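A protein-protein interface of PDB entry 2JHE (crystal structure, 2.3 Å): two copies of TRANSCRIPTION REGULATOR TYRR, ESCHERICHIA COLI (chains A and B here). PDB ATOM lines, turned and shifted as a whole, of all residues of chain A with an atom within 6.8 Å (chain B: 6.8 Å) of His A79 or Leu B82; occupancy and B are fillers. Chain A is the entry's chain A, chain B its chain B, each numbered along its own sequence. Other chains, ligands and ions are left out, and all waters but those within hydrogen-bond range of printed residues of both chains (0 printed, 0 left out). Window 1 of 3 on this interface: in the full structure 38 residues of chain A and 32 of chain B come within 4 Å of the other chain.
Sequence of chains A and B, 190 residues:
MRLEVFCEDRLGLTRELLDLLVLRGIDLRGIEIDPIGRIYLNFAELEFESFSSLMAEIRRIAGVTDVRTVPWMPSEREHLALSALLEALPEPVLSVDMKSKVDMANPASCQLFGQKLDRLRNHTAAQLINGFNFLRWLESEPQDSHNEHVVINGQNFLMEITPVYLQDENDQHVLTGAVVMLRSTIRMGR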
ATOM      1  N   SER A  75      27.117   8.370  -7.053  1.00  0.00           N
ATOM      2  CA  SER A  75      27.661   6.991  -6.865  1.00  0.00           C
ATOM      3  C   SER A  75      26.691   5.819  -7.182  1.00  0.00           C
ATOM      4  O   SER A  75      27.143   4.729  -7.505  1.00  0.00           O
ATOM      5  CB  SER A  75      28.179   6.815  -5.447  1.00  0.00           C
ATOM      6  OG  SER A  75      27.146   7.080  -4.500  1.00  0.00           O
ATOM      7  N   GLU A  76      25.376   6.053  -7.086  1.00  0.00           N
ATOM      8  CA  GLU A  76      24.356   4.985  -7.187  1.00  0.00           C
ATOM      9  C   GLU A  76      23.878   4.766  -8.607  1.00  0.00           C
ATOM     10  O   GLU A  76      23.332   3.723  -8.920  1.00  0.00           O
ATOM     11  CB  GLU A  76      23.108   5.309  -6.376  1.00  0.00           C
ATOM     12  CG  GLU A  76      23.357   5.467  -4.947  1.00  0.00           C
ATOM     13  CD  GLU A  76      22.117   5.721  -4.174  1.00  0.00           C
ATOM     14  OE1 GLU A  76      21.469   6.782  -4.347  1.00  0.00           O
ATOM     15  OE2 GLU A  76      21.789   4.851  -3.353  1.00  0.00           O
ATOM     16  N   ARG A  77      24.087   5.756  -9.459  1.00  0.00           N
ATOM     17  CA  ARG A  77      23.318   5.852 -10.697  1.00  0.00           C
ATOM     18  C   ARG A  77      23.387   4.609 -11.602  1.00  0.00           C
ATOM     19  O   ARG A  77      22.362   4.080 -11.994  1.00  0.00           O
ATOM     20  CB  ARG A  77      23.714   7.102 -11.458  1.00  0.00           C
ATOM     21  CG  ARG A  77      22.790   7.425 -12.612  1.00  0.00           C
ATOM     22  CD  ARG A  77      23.455   8.436 -13.494  1.00  0.00           C
ATOM     23  NE  ARG A  77      24.076   7.756 -14.632  1.00  0.00           N
ATOM     24  CZ  ARG A  77      25.378   7.705 -14.878  1.00  0.00           C
ATOM     25  NH1 ARG A  77      26.244   8.301 -14.081  1.00  0.00           N
ATOM     26  NH2 ARG A  77      25.810   7.049 -15.935  1.00  0.00           N
ATOM     27  N   GLU A  78      24.599   4.156 -11.882  1.00  0.00           N
ATOM     28  CA  GLU A  78      24.863   3.076 -12.797  1.00  0.00           C
ATOM     29  C   GLU A  78      24.501   1.723 -12.216  1.00  0.00           C
ATOM     30  O   GLU A  78      23.880   0.922 -12.891  1.00  0.00           O
ATOM     31  CB  GLU A  78      26.329   3.111 -13.203  1.00  0.00           C
ATOM     32  CG  GLU A  78      26.667   4.232 -14.185  1.00  0.00           C
ATOM     33  CD  GLU A  78      28.162   4.286 -14.541  1.00  0.00           C
ATOM     34  OE1 GLU A  78      28.958   3.490 -13.986  1.00  0.00           O
ATOM     35  OE2 GLU A  78      28.545   5.148 -15.368  1.00  0.00           O
ATOM     36  N   HIS A  79      24.860   1.459 -10.961  1.00  0.00           N
ATOM     37  CA  HIS A  79      24.495   0.197 -10.356  1.00  0.00           C
ATOM     38  C   HIS A  79      22.979   0.043 -10.163  1.00  0.00           C
ATOM     39  O   HIS A  79      22.476  -1.047 -10.133  1.00  0.00           O
ATOM     40  CB  HIS A  79      25.356  -0.159  -9.114  1.00  0.00           C
ATOM     41  CG  HIS A  79      24.925   0.485  -7.819  1.00  0.00           C
ATOM     42  ND1 HIS A  79      23.683   0.287  -7.257  1.00  0.00           N
ATOM     43  CD2 HIS A  79      25.620   1.227  -6.926  1.00  0.00           C
ATOM     44  CE1 HIS A  79      23.601   0.946  -6.115  1.00  0.00           C
ATOM     45  NE2 HIS A  79      24.775   1.505  -5.877  1.00  0.00           N
ATOM     46  N   LEU A  80      22.253   1.142 -10.092  1.00  0.00           N
ATOM     47  CA  LEU A  80      20.784   1.116 -10.013  1.00  0.00           C
ATOM     48  C   LEU A  80      20.157   0.852 -11.403  1.00  0.00           C
ATOM     49  O   LEU A  80      19.038   0.336 -11.500  1.00  0.00           O
ATOM     50  CB  LEU A  80      20.278   2.474  -9.487  1.00  0.00           C
ATOM     51  CG  LEU A  80      19.645   2.682  -8.103  1.00  0.00           C
ATOM     52  CD1 LEU A  80      20.001   1.717  -6.943  1.00  0.00           C
ATOM     53  CD2 LEU A  80      19.743   4.140  -7.678  1.00  0.00           C
ATOM     54  N   ALA A  81      20.853   1.254 -12.463  1.00  0.00           N
ATOM     55  CA  ALA A  81      20.413   0.991 -13.830  1.00  0.00           C
ATOM     56  C   ALA A  81      20.622  -0.503 -14.106  1.00  0.00           C
ATOM     57  O   ALA A  81      19.729  -1.203 -14.628  1.00  0.00           O
ATOM     58  CB  ALA A  81      21.173   1.835 -14.790  1.00  0.00           C
ATOM     59  N   LEU A  82      21.771  -1.017 -13.677  1.00  0.00           N
ATOM     60  CA  LEU A  82      21.990  -2.450 -13.751  1.00  0.00           C
ATOM     61  C   LEU A  82      20.962  -3.239 -12.983  1.00  0.00           C
ATOM     62  O   LEU A  82      20.402  -4.194 -13.527  1.00  0.00           O
ATOM     63  CB  LEU A  82      23.399  -2.829 -13.299  1.00  0.00           C
ATOM     64  CG  LEU A  82      24.454  -3.079 -14.351  1.00  0.00           C
ATOM     65  CD1 LEU A  82      24.100  -2.487 -15.722  1.00  0.00           C
ATOM     66  CD2 LEU A  82      25.807  -2.595 -13.829  1.00  0.00           C
ATOM     67  N   SER A  83      20.708  -2.878 -11.730  1.00  0.00           N
ATOM     68  CA  SER A  83      19.682  -3.583 -10.935  1.00  0.00           C
ATOM     69  C   SER A  83      18.282  -3.562 -11.556  1.00  0.00           C
ATOM     70  O   SER A  83      17.565  -4.591 -11.531  1.00  0.00           O
ATOM     71  CB  SER A  83      19.554  -2.953  -9.535  1.00  0.00           C
ATOM     72  OG  SER A  83      20.491  -3.535  -8.677  1.00  0.00           O
ATOM     73  N   ALA A  84      17.861  -2.387 -12.011  1.00  0.00           N
ATOM     74  CA  ALA A  84      16.579  -2.200 -12.682  1.00  0.00           C
ATOM     75  C   ALA A  84      16.382  -3.233 -13.826  1.00  0.00           C
ATOM     76  O   ALA A  84      15.356  -3.901 -13.872  1.00  0.00           O
ATOM     77  CB  ALA A  84      16.475  -0.782 -13.243  1.00  0.00           C
ATOM     78  N   LEU A  86      18.042  -6.108 -14.553  1.00  0.00           N
ATOM     79  CA  LEU A  86      17.953  -7.462 -13.980  1.00  0.00           C
ATOM     80  C   LEU A  86      16.692  -7.740 -13.185  1.00  0.00           C
ATOM     81  O   LEU A  86      16.249  -8.889 -13.076  1.00  0.00           O
ATOM     82  CB  LEU A  86      19.146  -7.762 -13.062  1.00  0.00           C
ATOM     83  CG  LEU A  86      20.524  -7.925 -13.680  1.00  0.00           C
ATOM     84  CD1 LEU A  86      21.549  -7.681 -12.585  1.00  0.00           C
ATOM     85  CD2 LEU A  86      20.684  -9.344 -14.335  1.00  0.00           C
ATOM     86  N   MET A 104      21.740 -11.930  -4.886  1.00  0.00           N
ATOM     87  CA  MET A 104      20.817 -11.225  -5.743  1.00  0.00           C
ATOM     88  C   MET A 104      19.698 -12.196  -6.085  1.00  0.00           C
ATOM     89  O   MET A 104      19.977 -13.355  -6.415  1.00  0.00           O
ATOM     90  CB  MET A 104      21.531 -10.737  -7.013  1.00  0.00           C
ATOM     91  CG  MET A 104      20.617  -9.997  -7.998  1.00  0.00           C
ATOM     92  SD  MET A 104      19.707 -11.033  -9.176  1.00  0.00           S
ATOM     93  CE  MET A 104      18.564  -9.824  -9.841  1.00  0.00           C
ATOM     94  N   PRO B  74      32.038   1.002  -1.238  1.00  0.00           N
ATOM     95  CA  PRO B  74      30.926   0.019  -1.356  1.00  0.00           C
ATOM     96  C   PRO B  74      30.044   0.169  -2.579  1.00  0.00           C
ATOM     97  O   PRO B  74      29.702  -0.831  -3.205  1.00  0.00           O
ATOM     98  CB  PRO B  74      30.112   0.220  -0.056  1.00  0.00           C
ATOM     99  CG  PRO B  74      31.187   0.667   0.936  1.00  0.00           C
ATOM    100  CD  PRO B  74      32.130   1.564   0.126  1.00  0.00           C
ATOM    101  N   SER B  75      29.631   1.368  -2.928  1.00  0.00           N
ATOM    102  CA  SER B  75      28.788   1.541  -4.129  1.00  0.00           C
ATOM    103  C   SER B  75      29.463   0.950  -5.398  1.00  0.00           C
ATOM    104  O   SER B  75      28.796   0.391  -6.246  1.00  0.00           O
ATOM    105  CB  SER B  75      28.546   3.019  -4.393  1.00  0.00           C
ATOM    106  OG  SER B  75      29.798   3.647  -4.467  1.00  0.00           O
ATOM    107  N   GLU B  76      30.775   1.096  -5.473  1.00  0.00           N
ATOM    108  CA  GLU B  76      31.601   0.618  -6.568  1.00  0.00           C
ATOM    109  C   GLU B  76      31.785  -0.902  -6.575  1.00  0.00           C
ATOM    110  O   GLU B  76      31.787  -1.502  -7.644  1.00  0.00           O
ATOM    111  CB  GLU B  76      32.965   1.290  -6.496  1.00  0.00           C
ATOM    112  CG  GLU B  76      33.026   2.735  -7.029  1.00  0.00           C
ATOM    113  CD  GLU B  76      34.392   3.340  -6.767  1.00  0.00           C
ATOM    114  OE1 GLU B  76      34.965   3.101  -5.679  1.00  0.00           O
ATOM    115  OE2 GLU B  76      34.913   4.094  -7.596  1.00  0.00           O
ATOM    116  N   ARG B  77      31.947  -1.508  -5.387  1.00  0.00           N
ATOM    117  CA  ARG B  77      31.874  -2.966  -5.224  1.00  0.00           C
ATOM    118  C   ARG B  77      30.525  -3.480  -5.687  1.00  0.00           C
ATOM    119  O   ARG B  77      30.511  -4.481  -6.390  1.00  0.00           O
ATOM    120  CB  ARG B  77      32.178  -3.458  -3.781  1.00  0.00           C
ATOM    121  CG  ARG B  77      33.586  -3.070  -3.222  1.00  0.00           C
ATOM    122  CD  ARG B  77      34.233  -4.239  -2.434  1.00  0.00           C
ATOM    123  NE  ARG B  77      35.708  -4.143  -2.334  1.00  0.00           N
ATOM    124  CZ  ARG B  77      36.585  -4.761  -3.128  1.00  0.00           C
ATOM    125  NH1 ARG B  77      36.191  -5.562  -4.114  1.00  0.00           N
ATOM    126  NH2 ARG B  77      37.881  -4.574  -2.927  1.00  0.00           N
ATOM    127  N   GLU B  78      29.410  -2.839  -5.264  1.00  0.00           N
ATOM    128  CA  GLU B  78      28.047  -3.175  -5.772  1.00  0.00           C
ATOM    129  C   GLU B  78      27.936  -3.126  -7.302  1.00  0.00           C
ATOM    130  O   GLU B  78      27.357  -4.006  -7.902  1.00  0.00           O
ATOM    131  CB  GLU B  78      26.967  -2.228  -5.256  1.00  0.00           C
ATOM    132  CG  GLU B  78      26.073  -2.761  -4.186  1.00  0.00           C
ATOM    133  CD  GLU B  78      25.085  -3.825  -4.669  1.00  0.00           C
ATOM    134  OE1 GLU B  78      23.958  -3.469  -5.127  1.00  0.00           O
ATOM    135  OE2 GLU B  78      25.432  -5.021  -4.541  1.00  0.00           O
ATOM    136  N   HIS B  79      28.435  -2.044  -7.897  1.00  0.00           N
ATOM    137  CA  HIS B  79      28.433  -1.905  -9.327  1.00  0.00           C
ATOM    138  C   HIS B  79      29.212  -3.076  -9.992  1.00  0.00           C
ATOM    139  O   HIS B  79      28.766  -3.647 -10.993  1.00  0.00           O
ATOM    140  CB  HIS B  79      28.983  -0.542  -9.722  1.00  0.00           C
ATOM    141  CG  HIS B  79      28.869  -0.239 -11.188  1.00  0.00           C
ATOM    142  ND1 HIS B  79      29.721   0.629 -11.841  1.00  0.00           N
ATOM    143  CD2 HIS B  79      28.008  -0.698 -12.136  1.00  0.00           C
ATOM    144  CE1 HIS B  79      29.394   0.695 -13.122  1.00  0.00           C
ATOM    145  NE2 HIS B  79      28.359  -0.104 -13.328  1.00  0.00           N
ATOM    146  N   LEU B  80      30.352  -3.443  -9.404  1.00  0.00           N
ATOM    147  CA  LEU B  80      31.156  -4.510  -9.942  1.00  0.00           C
ATOM    148  C   LEU B  80      30.462  -5.864  -9.897  1.00  0.00           C
ATOM    149  O   LEU B  80      30.530  -6.625 -10.865  1.00  0.00           O
ATOM    150  CB  LEU B  80      32.539  -4.562  -9.280  1.00  0.00           C
ATOM    151  CG  LEU B  80      33.477  -3.471  -9.796  1.00  0.00           C
ATOM    152  CD1 LEU B  80      34.599  -3.232  -8.782  1.00  0.00           C
ATOM    153  CD2 LEU B  80      34.045  -3.857 -11.162  1.00  0.00           C
ATOM    154  N   ALA B  81      29.818  -6.159  -8.776  1.00  0.00           N
ATOM    155  CA  ALA B  81      29.086  -7.416  -8.599  1.00  0.00           C
ATOM    156  C   ALA B  81      27.829  -7.558  -9.496  1.00  0.00           C
ATOM    157  O   ALA B  81      27.436  -8.655  -9.865  1.00  0.00           O
ATOM    158  CB  ALA B  81      28.709  -7.601  -7.132  1.00  0.00           C
ATOM    159  N   LEU B  82      27.193  -6.452  -9.826  1.00  0.00           N
ATOM    160  CA  LEU B  82      26.089  -6.455 -10.762  1.00  0.00           C
ATOM    161  C   LEU B  82      26.533  -6.531 -12.233  1.00  0.00           C
ATOM    162  O   LEU B  82      25.885  -7.216 -13.025  1.00  0.00           O
ATOM    163  CB  LEU B  82      25.152  -5.261 -10.517  1.00  0.00           C
ATOM    164  CG  LEU B  82      24.325  -5.358  -9.237  1.00  0.00           C
ATOM    165  CD1 LEU B  82      23.837  -3.971  -8.827  1.00  0.00           C
ATOM    166  CD2 LEU B  82      23.143  -6.388  -9.342  1.00  0.00           C
ATOM    167  N   SER B  83      27.613  -5.838 -12.583  1.00  0.00           N
ATOM    168  CA  SER B  83      28.222  -5.956 -13.902  1.00  0.00           C
ATOM    169  C   SER B  83      28.616  -7.387 -14.156  1.00  0.00           C
ATOM    170  O   SER B  83      28.441  -7.859 -15.246  1.00  0.00           O
ATOM    171  CB  SER B  83      29.485  -5.121 -14.020  1.00  0.00           C
ATOM    172  OG  SER B  83      29.155  -3.765 -14.166  1.00  0.00           O
ATOM    173  N   ALA B  84      29.157  -8.056 -13.135  1.00  0.00           N
ATOM    174  CA  ALA B  84      29.625  -9.450 -13.239  1.00  0.00           C
ATOM    175  C   ALA B  84      28.507 -10.457 -13.495  1.00  0.00           C
ATOM    176  O   ALA B  84      28.727 -11.407 -14.257  1.00  0.00           O
ATOM    177  CB  ALA B  84      30.450  -9.853 -12.005  1.00  0.00           C
ATOM    178  N   LEU B  85      27.338 -10.264 -12.860  1.00  0.00           N
ATOM    179  CA  LEU B  85      26.135 -11.094 -13.143  1.00  0.00           C
ATOM    180  C   LEU B  85      25.717 -10.910 -14.609  1.00  0.00           C
ATOM    181  O   LEU B  85      25.705 -11.849 -15.371  1.00  0.00           O
ATOM    182  CB  LEU B  85      24.938 -10.787 -12.218  1.00  0.00           C
ATOM    183  CG  LEU B  85      24.964 -11.011 -10.696  1.00  0.00           C
ATOM    184  CD1 LEU B  85      23.592 -10.716 -10.122  1.00  0.00           C
ATOM    185  CD2 LEU B  85      25.383 -12.409 -10.285  1.00  0.00           C
ATOM    186  N   LEU B  86      25.410  -9.676 -14.984  1.00  0.00           N
ATOM    187  CA  LEU B  86      25.114  -9.354 -16.344  1.00  0.00           C
ATOM    188  C   LEU B  86      26.124  -9.942 -17.368  1.00  0.00           C
ATOM    189  O   LEU B  86      25.705 -10.483 -18.409  1.00  0.00           O
ATOM    190  CB  LEU B  86      24.958  -7.844 -16.519  1.00  0.00           C
ATOM    191  CG  LEU B  86      24.905  -7.408 -17.989  1.00  0.00           C
ATOM    192  CD1 LEU B  86      23.713  -7.993 -18.779  1.00  0.00           C
ATOM    193  CD2 LEU B  86      24.961  -5.911 -18.116  1.00  0.00           C
ATOM    194  N   GLU B  87      27.417  -9.814 -17.107  1.00  0.00           N
ATOM    195  CA  GLU B  87      28.423 -10.298 -18.064  1.00  0.00           C
ATOM    196  C   GLU B  87      28.533 -11.827 -18.096  1.00  0.00           C
ATOM    197  O   GLU B  87      28.930 -12.393 -19.117  1.00  0.00           O
ATOM    198  CB  GLU B  87      29.785  -9.658 -17.807  1.00  0.00           C
ATOM    199  CG  GLU B  87      29.826  -8.139 -18.126  1.00  0.00           C
ATOM    200  CD  GLU B  87      30.938  -7.424 -17.383  1.00  0.00           C
ATOM    201  OE1 GLU B  87      31.663  -8.106 -16.621  1.00  0.00           O
ATOM    202  OE2 GLU B  87      31.081  -6.187 -17.547  1.00  0.00           O
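Glu A78 touches His B79, but with the chains exchanged His A79 does not touch Glu B78 (4.1 Å).
His A79 touches Ser B75, but with the chains exchanged Ser A75 does not touch His B79 (6.0 Å).
His B79 touches its own counterpart, His A79.
Leu A82 touches Ser B83, and with the chains exchanged Ser A83 touches Leu B82.
11 positions are printed for both chains.
His A79 touches three residues of chain B.
Printed residues of chain A within 4 Å of Ser B75: Ser A75 and His A79.
Of the printed residues of chain B, Leu A82 touches His B79 and Ser B83.
Of the printed residues of chain B, Ser A75 touches Ser B75.
Printed residues of chain B within 4 Å of Glu A78: His B79 (3.0 Å).
The nearest residue of chain A that does not touch Leu B82 is Leu A82 (4.1 Å).
Ser B75 touches Ser A75 (OG to CB, 3.7 Å).
Glu A78 touches His B79 (OE1 to CE1, 3.0 Å).
O of Ser B75 touches CD2 of His A79, at 3.4 Å.
CB of His A79 touches CA of His B79, 3.5 Å away.
His A79 touches Leu B82 (O to CD1, 3.5 Å).
CD2 of His B79 touches CD2 of Leu A82 (3.4 Å).
OG of Ser B83 touches CD2 of Leu A82, at 3.6 Å.
OG of Ser A83 touches CD1 of Leu B82, 3.4 Å away.
Leu A86 touches Leu B82 (CD1 to CD2, 3.8 Å).
Leu B85 touches Met A104.
Of the 12 printed residues of chain A, 7 touch a printed residue of chain B.
Printed residues of chain B that touch a printed residue of chain A: Ser B75, His B79, Leu B82, Ser B83 and Leu B85.
Hydrophobic or aromatic side chains of chain B that line the printed part of chain A: His B79, Leu B82 and Leu B85.
Among the printed residues, 10 pairs touch across the chains.
Among the printed residues, no Asp or Glu carboxylate lies within 4 Å of a Lys or Arg side-chain nitrogen of the other chain.
O of His B79 is in hydrogen-bond range of OG of Ser B83.
The guanidinium group of Arg A77 is in salt-bridge range of the side-chain carboxylate of Glu A78.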
